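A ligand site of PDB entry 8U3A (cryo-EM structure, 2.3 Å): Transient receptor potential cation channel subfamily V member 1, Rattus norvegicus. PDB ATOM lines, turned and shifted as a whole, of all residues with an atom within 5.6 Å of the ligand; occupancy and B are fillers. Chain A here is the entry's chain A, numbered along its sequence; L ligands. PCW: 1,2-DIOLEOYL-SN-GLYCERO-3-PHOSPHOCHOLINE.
CG1 of Val 334 touches C3 of the ligand, 3.6 Å away. Leu 337 touches the ligand (CB to C38, 3.7 Å). N of Tyr 338 touches C38 of the ligand (3.3 Å). Gly 378 touches the ligand (CA to C33, 3.8 Å). Tyr 381 touches the ligand (CE2 to O2, 3.3 Å). CZ of Phe 382 touches O31 of the ligand (3.3 Å). Glu 407 touches the ligand. Phe 410 touches the ligand. CE2 of Tyr 448 touches C4 of the ligand, 3.8 Å away.
NH1 of Arg 385 lies within salt-bridge range of O2P of the ligand, at 3.2 Å. O4P of the ligand lies within hydrogen-bond range of OH of Tyr 449, at 2.7 Å. OD1 of Asn 331 lies close to O11 of the ligand, 3.1 Å away.
The guanidinium group (NH1) of Arg 385 lies within hydrogen-bond range of the side-chain hydroxyl (OH) of Tyr 381 (2.8 Å).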
ATOM      1  N   PHE A 330      -1.380  -9.587  14.629  1.00  0.00           N
ATOM      2  CA  PHE A 330      -0.106  -8.885  14.767  1.00  0.00           C
ATOM      3  C   PHE A 330      -0.003  -8.191  16.131  1.00  0.00           C
ATOM      4  O   PHE A 330       1.054  -8.208  16.770  1.00  0.00           O
ATOM      5  CB  PHE A 330       0.075  -7.867  13.643  1.00  0.00           C
ATOM      6  CG  PHE A 330       1.372  -7.119  13.717  1.00  0.00           C
ATOM      7  CD1 PHE A 330       2.549  -7.698  13.296  1.00  0.00           C
ATOM      8  CD2 PHE A 330       1.415  -5.825  14.215  1.00  0.00           C
ATOM      9  CE1 PHE A 330       3.744  -7.016  13.367  1.00  0.00           C
ATOM     10  CE2 PHE A 330       2.599  -5.135  14.287  1.00  0.00           C
ATOM     11  CZ  PHE A 330       3.766  -5.727  13.860  1.00  0.00           C
ATOM     12  N   ASN A 331      -1.096  -7.571  16.578  1.00  0.00           N
ATOM     13  CA  ASN A 331      -1.100  -6.936  17.894  1.00  0.00           C
ATOM     14  C   ASN A 331      -0.846  -7.962  18.997  1.00  0.00           C
ATOM     15  O   ASN A 331      -0.090  -7.708  19.934  1.00  0.00           O
ATOM     16  CB  ASN A 331      -2.415  -6.214  18.129  1.00  0.00           C
ATOM     17  CG  ASN A 331      -2.563  -4.986  17.265  1.00  0.00           C
ATOM     18  OD1 ASN A 331      -1.587  -4.453  16.732  1.00  0.00           O
ATOM     19  ND2 ASN A 331      -3.796  -4.504  17.117  1.00  0.00           N
ATOM     20  N   VAL A 334       2.821  -8.931  19.002  1.00  0.00           N
ATOM     21  CA  VAL A 334       3.652  -7.883  19.577  1.00  0.00           C
ATOM     22  C   VAL A 334       3.518  -7.872  21.096  1.00  0.00           C
ATOM     23  O   VAL A 334       4.515  -7.712  21.817  1.00  0.00           O
ATOM     24  CB  VAL A 334       3.291  -6.515  18.968  1.00  0.00           C
ATOM     25  CG1 VAL A 334       3.909  -5.385  19.770  1.00  0.00           C
ATOM     26  CG2 VAL A 334       3.745  -6.455  17.525  1.00  0.00           C
ATOM     27  N   TYR A 335       2.300  -8.028  21.601  1.00  0.00           N
ATOM     28  CA  TYR A 335       2.098  -8.046  23.052  1.00  0.00           C
ATOM     29  C   TYR A 335       2.789  -9.245  23.684  1.00  0.00           C
ATOM     30  O   TYR A 335       3.353  -9.139  24.779  1.00  0.00           O
ATOM     31  CB  TYR A 335       0.622  -8.045  23.393  1.00  0.00           C
ATOM     32  CG  TYR A 335       0.369  -7.907  24.875  1.00  0.00           C
ATOM     33  CD1 TYR A 335       0.612  -6.706  25.528  1.00  0.00           C
ATOM     34  CD2 TYR A 335      -0.106  -8.972  25.617  1.00  0.00           C
ATOM     35  CE1 TYR A 335       0.382  -6.578  26.882  1.00  0.00           C
ATOM     36  CE2 TYR A 335      -0.340  -8.851  26.977  1.00  0.00           C
ATOM     37  CZ  TYR A 335      -0.090  -7.651  27.600  1.00  0.00           C
ATOM     38  OH  TYR A 335      -0.317  -7.531  28.948  1.00  0.00           O
ATOM     39  N   LEU A 337       5.484 -10.750  22.576  1.00  0.00           N
ATOM     40  CA  LEU A 337       6.911 -10.430  22.599  1.00  0.00           C
ATOM     41  C   LEU A 337       7.232  -9.456  23.735  1.00  0.00           C
ATOM     42  O   LEU A 337       8.237  -9.616  24.428  1.00  0.00           O
ATOM     43  CB  LEU A 337       7.355  -9.842  21.259  1.00  0.00           C
ATOM     44  CG  LEU A 337       7.561 -10.820  20.111  1.00  0.00           C
ATOM     45  CD1 LEU A 337       7.951 -10.047  18.864  1.00  0.00           C
ATOM     46  CD2 LEU A 337       8.620 -11.864  20.446  1.00  0.00           C
ATOM     47  N   TYR A 338       6.388  -8.440  23.907  1.00  0.00           N
ATOM     48  CA  TYR A 338       6.612  -7.462  24.971  1.00  0.00           C
ATOM     49  C   TYR A 338       6.599  -8.135  26.337  1.00  0.00           C
ATOM     50  O   TYR A 338       7.453  -7.865  27.184  1.00  0.00           O
ATOM     51  CB  TYR A 338       5.551  -6.373  24.902  1.00  0.00           C
ATOM     52  CG  TYR A 338       5.422  -5.546  26.147  1.00  0.00           C
ATOM     53  CD1 TYR A 338       6.418  -4.647  26.520  1.00  0.00           C
ATOM     54  CD2 TYR A 338       4.312  -5.655  26.972  1.00  0.00           C
ATOM     55  CE1 TYR A 338       6.302  -3.893  27.660  1.00  0.00           C
ATOM     56  CE2 TYR A 338       4.183  -4.907  28.113  1.00  0.00           C
ATOM     57  CZ  TYR A 338       5.185  -4.023  28.457  1.00  0.00           C
ATOM     58  OH  TYR A 338       5.064  -3.276  29.603  1.00  0.00           O
ATOM     59  N   ILE A 341       9.767 -10.275  26.848  1.00  0.00           N
ATOM     60  CA  ILE A 341      10.944  -9.461  27.134  1.00  0.00           C
ATOM     61  C   ILE A 341      10.866  -8.881  28.534  1.00  0.00           C
ATOM     62  O   ILE A 341      11.877  -8.821  29.255  1.00  0.00           O
ATOM     63  CB  ILE A 341      11.107  -8.362  26.069  1.00  0.00           C
ATOM     64  CG1 ILE A 341      11.616  -8.970  24.758  1.00  0.00           C
ATOM     65  CG2 ILE A 341      12.066  -7.281  26.546  1.00  0.00           C
ATOM     66  CD1 ILE A 341      11.308  -8.131  23.542  1.00  0.00           C
ATOM     67  N   LEU A 374      12.918  -1.534  26.728  1.00  0.00           N
ATOM     68  CA  LEU A 374      11.719  -1.906  25.985  1.00  0.00           C
ATOM     69  C   LEU A 374      10.511  -2.032  26.900  1.00  0.00           C
ATOM     70  O   LEU A 374       9.406  -1.630  26.546  1.00  0.00           O
ATOM     71  CB  LEU A 374      11.953  -3.219  25.229  1.00  0.00           C
ATOM     72  CG  LEU A 374      13.027  -3.193  24.134  1.00  0.00           C
ATOM     73  CD1 LEU A 374      13.168  -4.565  23.508  1.00  0.00           C
ATOM     74  CD2 LEU A 374      12.686  -2.157  23.075  1.00  0.00           C
ATOM     75  N   SER A 377       9.359   1.422  27.747  1.00  0.00           N
ATOM     76  CA  SER A 377       8.733   2.021  26.572  1.00  0.00           C
ATOM     77  C   SER A 377       7.321   1.491  26.381  1.00  0.00           C
ATOM     78  O   SER A 377       6.398   2.257  26.065  1.00  0.00           O
ATOM     79  CB  SER A 377       9.587   1.744  25.341  1.00  0.00           C
ATOM     80  OG  SER A 377       9.524   0.382  24.971  1.00  0.00           O
ATOM     81  N   GLY A 378       7.123   0.184  26.553  1.00  0.00           N
ATOM     82  CA  GLY A 378       5.789  -0.376  26.457  1.00  0.00           C
ATOM     83  C   GLY A 378       4.861   0.165  27.534  1.00  0.00           C
ATOM     84  O   GLY A 378       3.676   0.420  27.274  1.00  0.00           O
ATOM     85  N   TYR A 381       3.862   3.568  26.463  1.00  0.00           N
ATOM     86  CA  TYR A 381       2.943   3.403  25.312  1.00  0.00           C
ATOM     87  C   TYR A 381       1.535   3.098  25.807  1.00  0.00           C
ATOM     88  O   TYR A 381       0.599   3.643  25.238  1.00  0.00           O
ATOM     89  CB  TYR A 381       3.368   2.259  24.404  1.00  0.00           C
ATOM     90  CG  TYR A 381       2.295   1.807  23.438  1.00  0.00           C
ATOM     91  CD1 TYR A 381       1.903   2.620  22.381  1.00  0.00           C
ATOM     92  CD2 TYR A 381       1.636   0.602  23.614  1.00  0.00           C
ATOM     93  CE1 TYR A 381       0.913   2.216  21.498  1.00  0.00           C
ATOM     94  CE2 TYR A 381       0.647   0.198  22.749  1.00  0.00           C
ATOM     95  CZ  TYR A 381       0.282   1.001  21.685  1.00  0.00           C
ATOM     96  OH  TYR A 381      -0.707   0.597  20.820  1.00  0.00           O
ATOM     97  N   PHE A 382       1.405   2.201  26.784  1.00  0.00           N
ATOM     98  CA  PHE A 382       0.086   1.836  27.300  1.00  0.00           C
ATOM     99  C   PHE A 382      -0.517   2.957  28.144  1.00  0.00           C
ATOM    100  O   PHE A 382      -1.725   3.181  28.117  1.00  0.00           O
ATOM    101  CB  PHE A 382       0.170   0.536  28.103  1.00  0.00           C
ATOM    102  CG  PHE A 382       0.212  -0.699  27.249  1.00  0.00           C
ATOM    103  CD1 PHE A 382      -0.801  -0.966  26.332  1.00  0.00           C
ATOM    104  CD2 PHE A 382       1.264  -1.587  27.347  1.00  0.00           C
ATOM    105  CE1 PHE A 382      -0.765  -2.092  25.542  1.00  0.00           C
ATOM    106  CE2 PHE A 382       1.296  -2.721  26.563  1.00  0.00           C
ATOM    107  CZ  PHE A 382       0.285  -2.974  25.663  1.00  0.00           C
ATOM    108  N   ARG A 385      -1.844   5.421  25.701  1.00  0.00           N
ATOM    109  CA  ARG A 385      -3.012   4.817  24.998  1.00  0.00           C
ATOM    110  C   ARG A 385      -4.219   4.869  25.925  1.00  0.00           C
ATOM    111  O   ARG A 385      -5.324   5.007  25.397  1.00  0.00           O
ATOM    112  CB  ARG A 385      -2.723   3.372  24.593  1.00  0.00           C
ATOM    113  CG  ARG A 385      -1.961   3.212  23.284  1.00  0.00           C
ATOM    114  CD  ARG A 385      -2.772   3.610  22.064  1.00  0.00           C
ATOM    115  NE  ARG A 385      -4.097   3.001  22.037  1.00  0.00           N
ATOM    116  CZ  ARG A 385      -4.332   1.689  21.991  1.00  0.00           C
ATOM    117  NH1 ARG A 385      -3.420   0.849  21.545  1.00  0.00           N
ATOM    118  NH2 ARG A 385      -5.506   1.229  22.380  1.00  0.00           N
ATOM    119  N   SER A 406     -11.052  -3.699  30.358  1.00  0.00           N
ATOM    120  CA  SER A 406      -9.750  -3.931  29.677  1.00  0.00           C
ATOM    121  C   SER A 406      -8.918  -2.646  29.708  1.00  0.00           C
ATOM    122  O   SER A 406      -7.761  -2.741  30.089  1.00  0.00           O
ATOM    123  CB  SER A 406      -9.942  -4.424  28.264  1.00  0.00           C
ATOM    124  OG  SER A 406     -10.738  -3.526  27.504  1.00  0.00           O
ATOM    125  N   GLU A 407      -9.499  -1.500  29.339  1.00  0.00           N
ATOM    126  CA  GLU A 407      -8.768  -0.239  29.281  1.00  0.00           C
ATOM    127  C   GLU A 407      -8.208   0.133  30.647  1.00  0.00           C
ATOM    128  O   GLU A 407      -7.038   0.505  30.778  1.00  0.00           O
ATOM    129  CB  GLU A 407      -9.678   0.873  28.750  1.00  0.00           C
ATOM    130  CG  GLU A 407      -9.924   0.799  27.251  1.00  0.00           C
ATOM    131  CD  GLU A 407      -8.702   1.166  26.427  1.00  0.00           C
ATOM    132  OE1 GLU A 407      -7.724   1.663  27.015  1.00  0.00           O
ATOM    133  OE2 GLU A 407      -8.731   0.969  25.198  1.00  0.00           O
ATOM    134  N   PHE A 410      -5.228  -2.338  31.588  1.00  0.00           N
ATOM    135  CA  PHE A 410      -3.984  -2.008  30.907  1.00  0.00           C
ATOM    136  C   PHE A 410      -3.400  -0.698  31.427  1.00  0.00           C
ATOM    137  O   PHE A 410      -2.186  -0.566  31.614  1.00  0.00           O
ATOM    138  CB  PHE A 410      -4.218  -1.934  29.396  1.00  0.00           C
ATOM    139  CG  PHE A 410      -4.173  -3.268  28.704  1.00  0.00           C
ATOM    140  CD1 PHE A 410      -5.272  -4.110  28.734  1.00  0.00           C
ATOM    141  CD2 PHE A 410      -3.039  -3.680  28.030  1.00  0.00           C
ATOM    142  CE1 PHE A 410      -5.237  -5.328  28.094  1.00  0.00           C
ATOM    143  CE2 PHE A 410      -3.001  -4.906  27.402  1.00  0.00           C
ATOM    144  CZ  PHE A 410      -4.098  -5.733  27.431  1.00  0.00           C
ATOM    145  N   TYR A 448      -7.115 -10.690  27.417  1.00  0.00           N
ATOM    146  CA  TYR A 448      -7.828  -9.759  26.538  1.00  0.00           C
ATOM    147  C   TYR A 448      -7.869 -10.284  25.108  1.00  0.00           C
ATOM    148  O   TYR A 448      -8.882 -10.122  24.410  1.00  0.00           O
ATOM    149  CB  TYR A 448      -7.159  -8.384  26.575  1.00  0.00           C
ATOM    150  CG  TYR A 448      -7.598  -7.487  25.439  1.00  0.00           C
ATOM    151  CD1 TYR A 448      -8.719  -6.689  25.540  1.00  0.00           C
ATOM    152  CD2 TYR A 448      -6.873  -7.442  24.257  1.00  0.00           C
ATOM    153  CE1 TYR A 448      -9.118  -5.874  24.512  1.00  0.00           C
ATOM    154  CE2 TYR A 448      -7.264  -6.629  23.218  1.00  0.00           C
ATOM    155  CZ  TYR A 448      -8.383  -5.852  23.348  1.00  0.00           C
ATOM    156  OH  TYR A 448      -8.774  -5.038  22.308  1.00  0.00           O
ATOM    157  N   TYR A 449      -6.797 -10.908  24.656  1.00  0.00           N
ATOM    158  CA  TYR A 449      -6.694 -11.348  23.279  1.00  0.00           C
ATOM    159  C   TYR A 449      -7.437 -12.646  23.002  1.00  0.00           C
ATOM    160  O   TYR A 449      -7.386 -13.143  21.875  1.00  0.00           O
ATOM    161  CB  TYR A 449      -5.215 -11.485  22.892  1.00  0.00           C
ATOM    162  CG  TYR A 449      -4.496 -10.159  22.863  1.00  0.00           C
ATOM    163  CD1 TYR A 449      -4.587  -9.330  21.755  1.00  0.00           C
ATOM    164  CD2 TYR A 449      -3.744  -9.740  23.945  1.00  0.00           C
ATOM    165  CE1 TYR A 449      -3.943  -8.115  21.729  1.00  0.00           C
ATOM    166  CE2 TYR A 449      -3.102  -8.518  23.925  1.00  0.00           C
ATOM    167  CZ  TYR A 449      -3.197  -7.717  22.817  1.00  0.00           C
ATOM    168  OH  TYR A 449      -2.552  -6.503  22.791  1.00  0.00           O
HETATM  169  C1  PCW L   1      -0.606  -4.447  21.955  1.00  0.00           C
HETATM  170  C2  PCW L   1       0.760  -4.123  21.380  1.00  0.00           C
HETATM  171  C3  PCW L   1       0.590  -3.928  19.884  1.00  0.00           C
HETATM  172  C4  PCW L   1      -4.742  -3.958  24.110  1.00  0.00           C
HETATM  173  C5  PCW L   1      -4.701  -2.655  24.903  1.00  0.00           C
HETATM  174  C6  PCW L   1      -6.791  -2.522  26.068  1.00  0.00           C
HETATM  175  C7  PCW L   1      -5.574  -0.616  25.437  1.00  0.00           C
HETATM  176  C8  PCW L   1      -6.720  -1.861  23.811  1.00  0.00           C
HETATM  177  C11 PCW L   1       1.079  -2.193  18.412  1.00  0.00           C
HETATM  178  C12 PCW L   1       2.477  -1.570  18.477  1.00  0.00           C
HETATM  179  C13 PCW L   1       3.360  -2.184  17.402  1.00  0.00           C
HETATM  180  C14 PCW L   1       4.767  -1.611  17.535  1.00  0.00           C
HETATM  181  C31 PCW L   1       2.487  -3.025  22.611  1.00  0.00           C
HETATM  182  C32 PCW L   1       3.636  -2.164  22.054  1.00  0.00           C
HETATM  183  C33 PCW L   1       4.720  -1.926  23.113  1.00  0.00           C
HETATM  184  C34 PCW L   1       5.626  -3.154  23.193  1.00  0.00           C
HETATM  185  C35 PCW L   1       7.035  -2.792  22.779  1.00  0.00           C
HETATM  186  C36 PCW L   1       7.935  -4.019  22.923  1.00  0.00           C
HETATM  187  C37 PCW L   1       7.974  -4.786  21.607  1.00  0.00           C
HETATM  188  C38 PCW L   1       7.923  -6.280  21.889  1.00  0.00           C
HETATM  189  N   PCW L   1      -5.959  -1.948  25.032  1.00  0.00           N
HETATM  190  O2  PCW L   1       1.214  -2.933  21.985  1.00  0.00           O
HETATM  191  O3  PCW L   1       0.423  -2.573  19.597  1.00  0.00           O
HETATM  192  O11 PCW L   1       0.559  -2.361  17.368  1.00  0.00           O
HETATM  193  O31 PCW L   1       2.646  -3.756  23.543  1.00  0.00           O
HETATM  194  O1P PCW L   1      -3.646  -4.382  21.011  1.00  0.00           O
HETATM  195  O2P PCW L   1      -3.806  -2.280  21.751  1.00  0.00           O
HETATM  196  O3P PCW L   1      -1.449  -3.312  21.872  1.00  0.00           O
HETATM  197  O4P PCW L   1      -3.448  -4.089  23.568  1.00  0.00           O
HETATM  198  P   PCW L   1      -3.093  -3.506  22.052  1.00  0.00           P
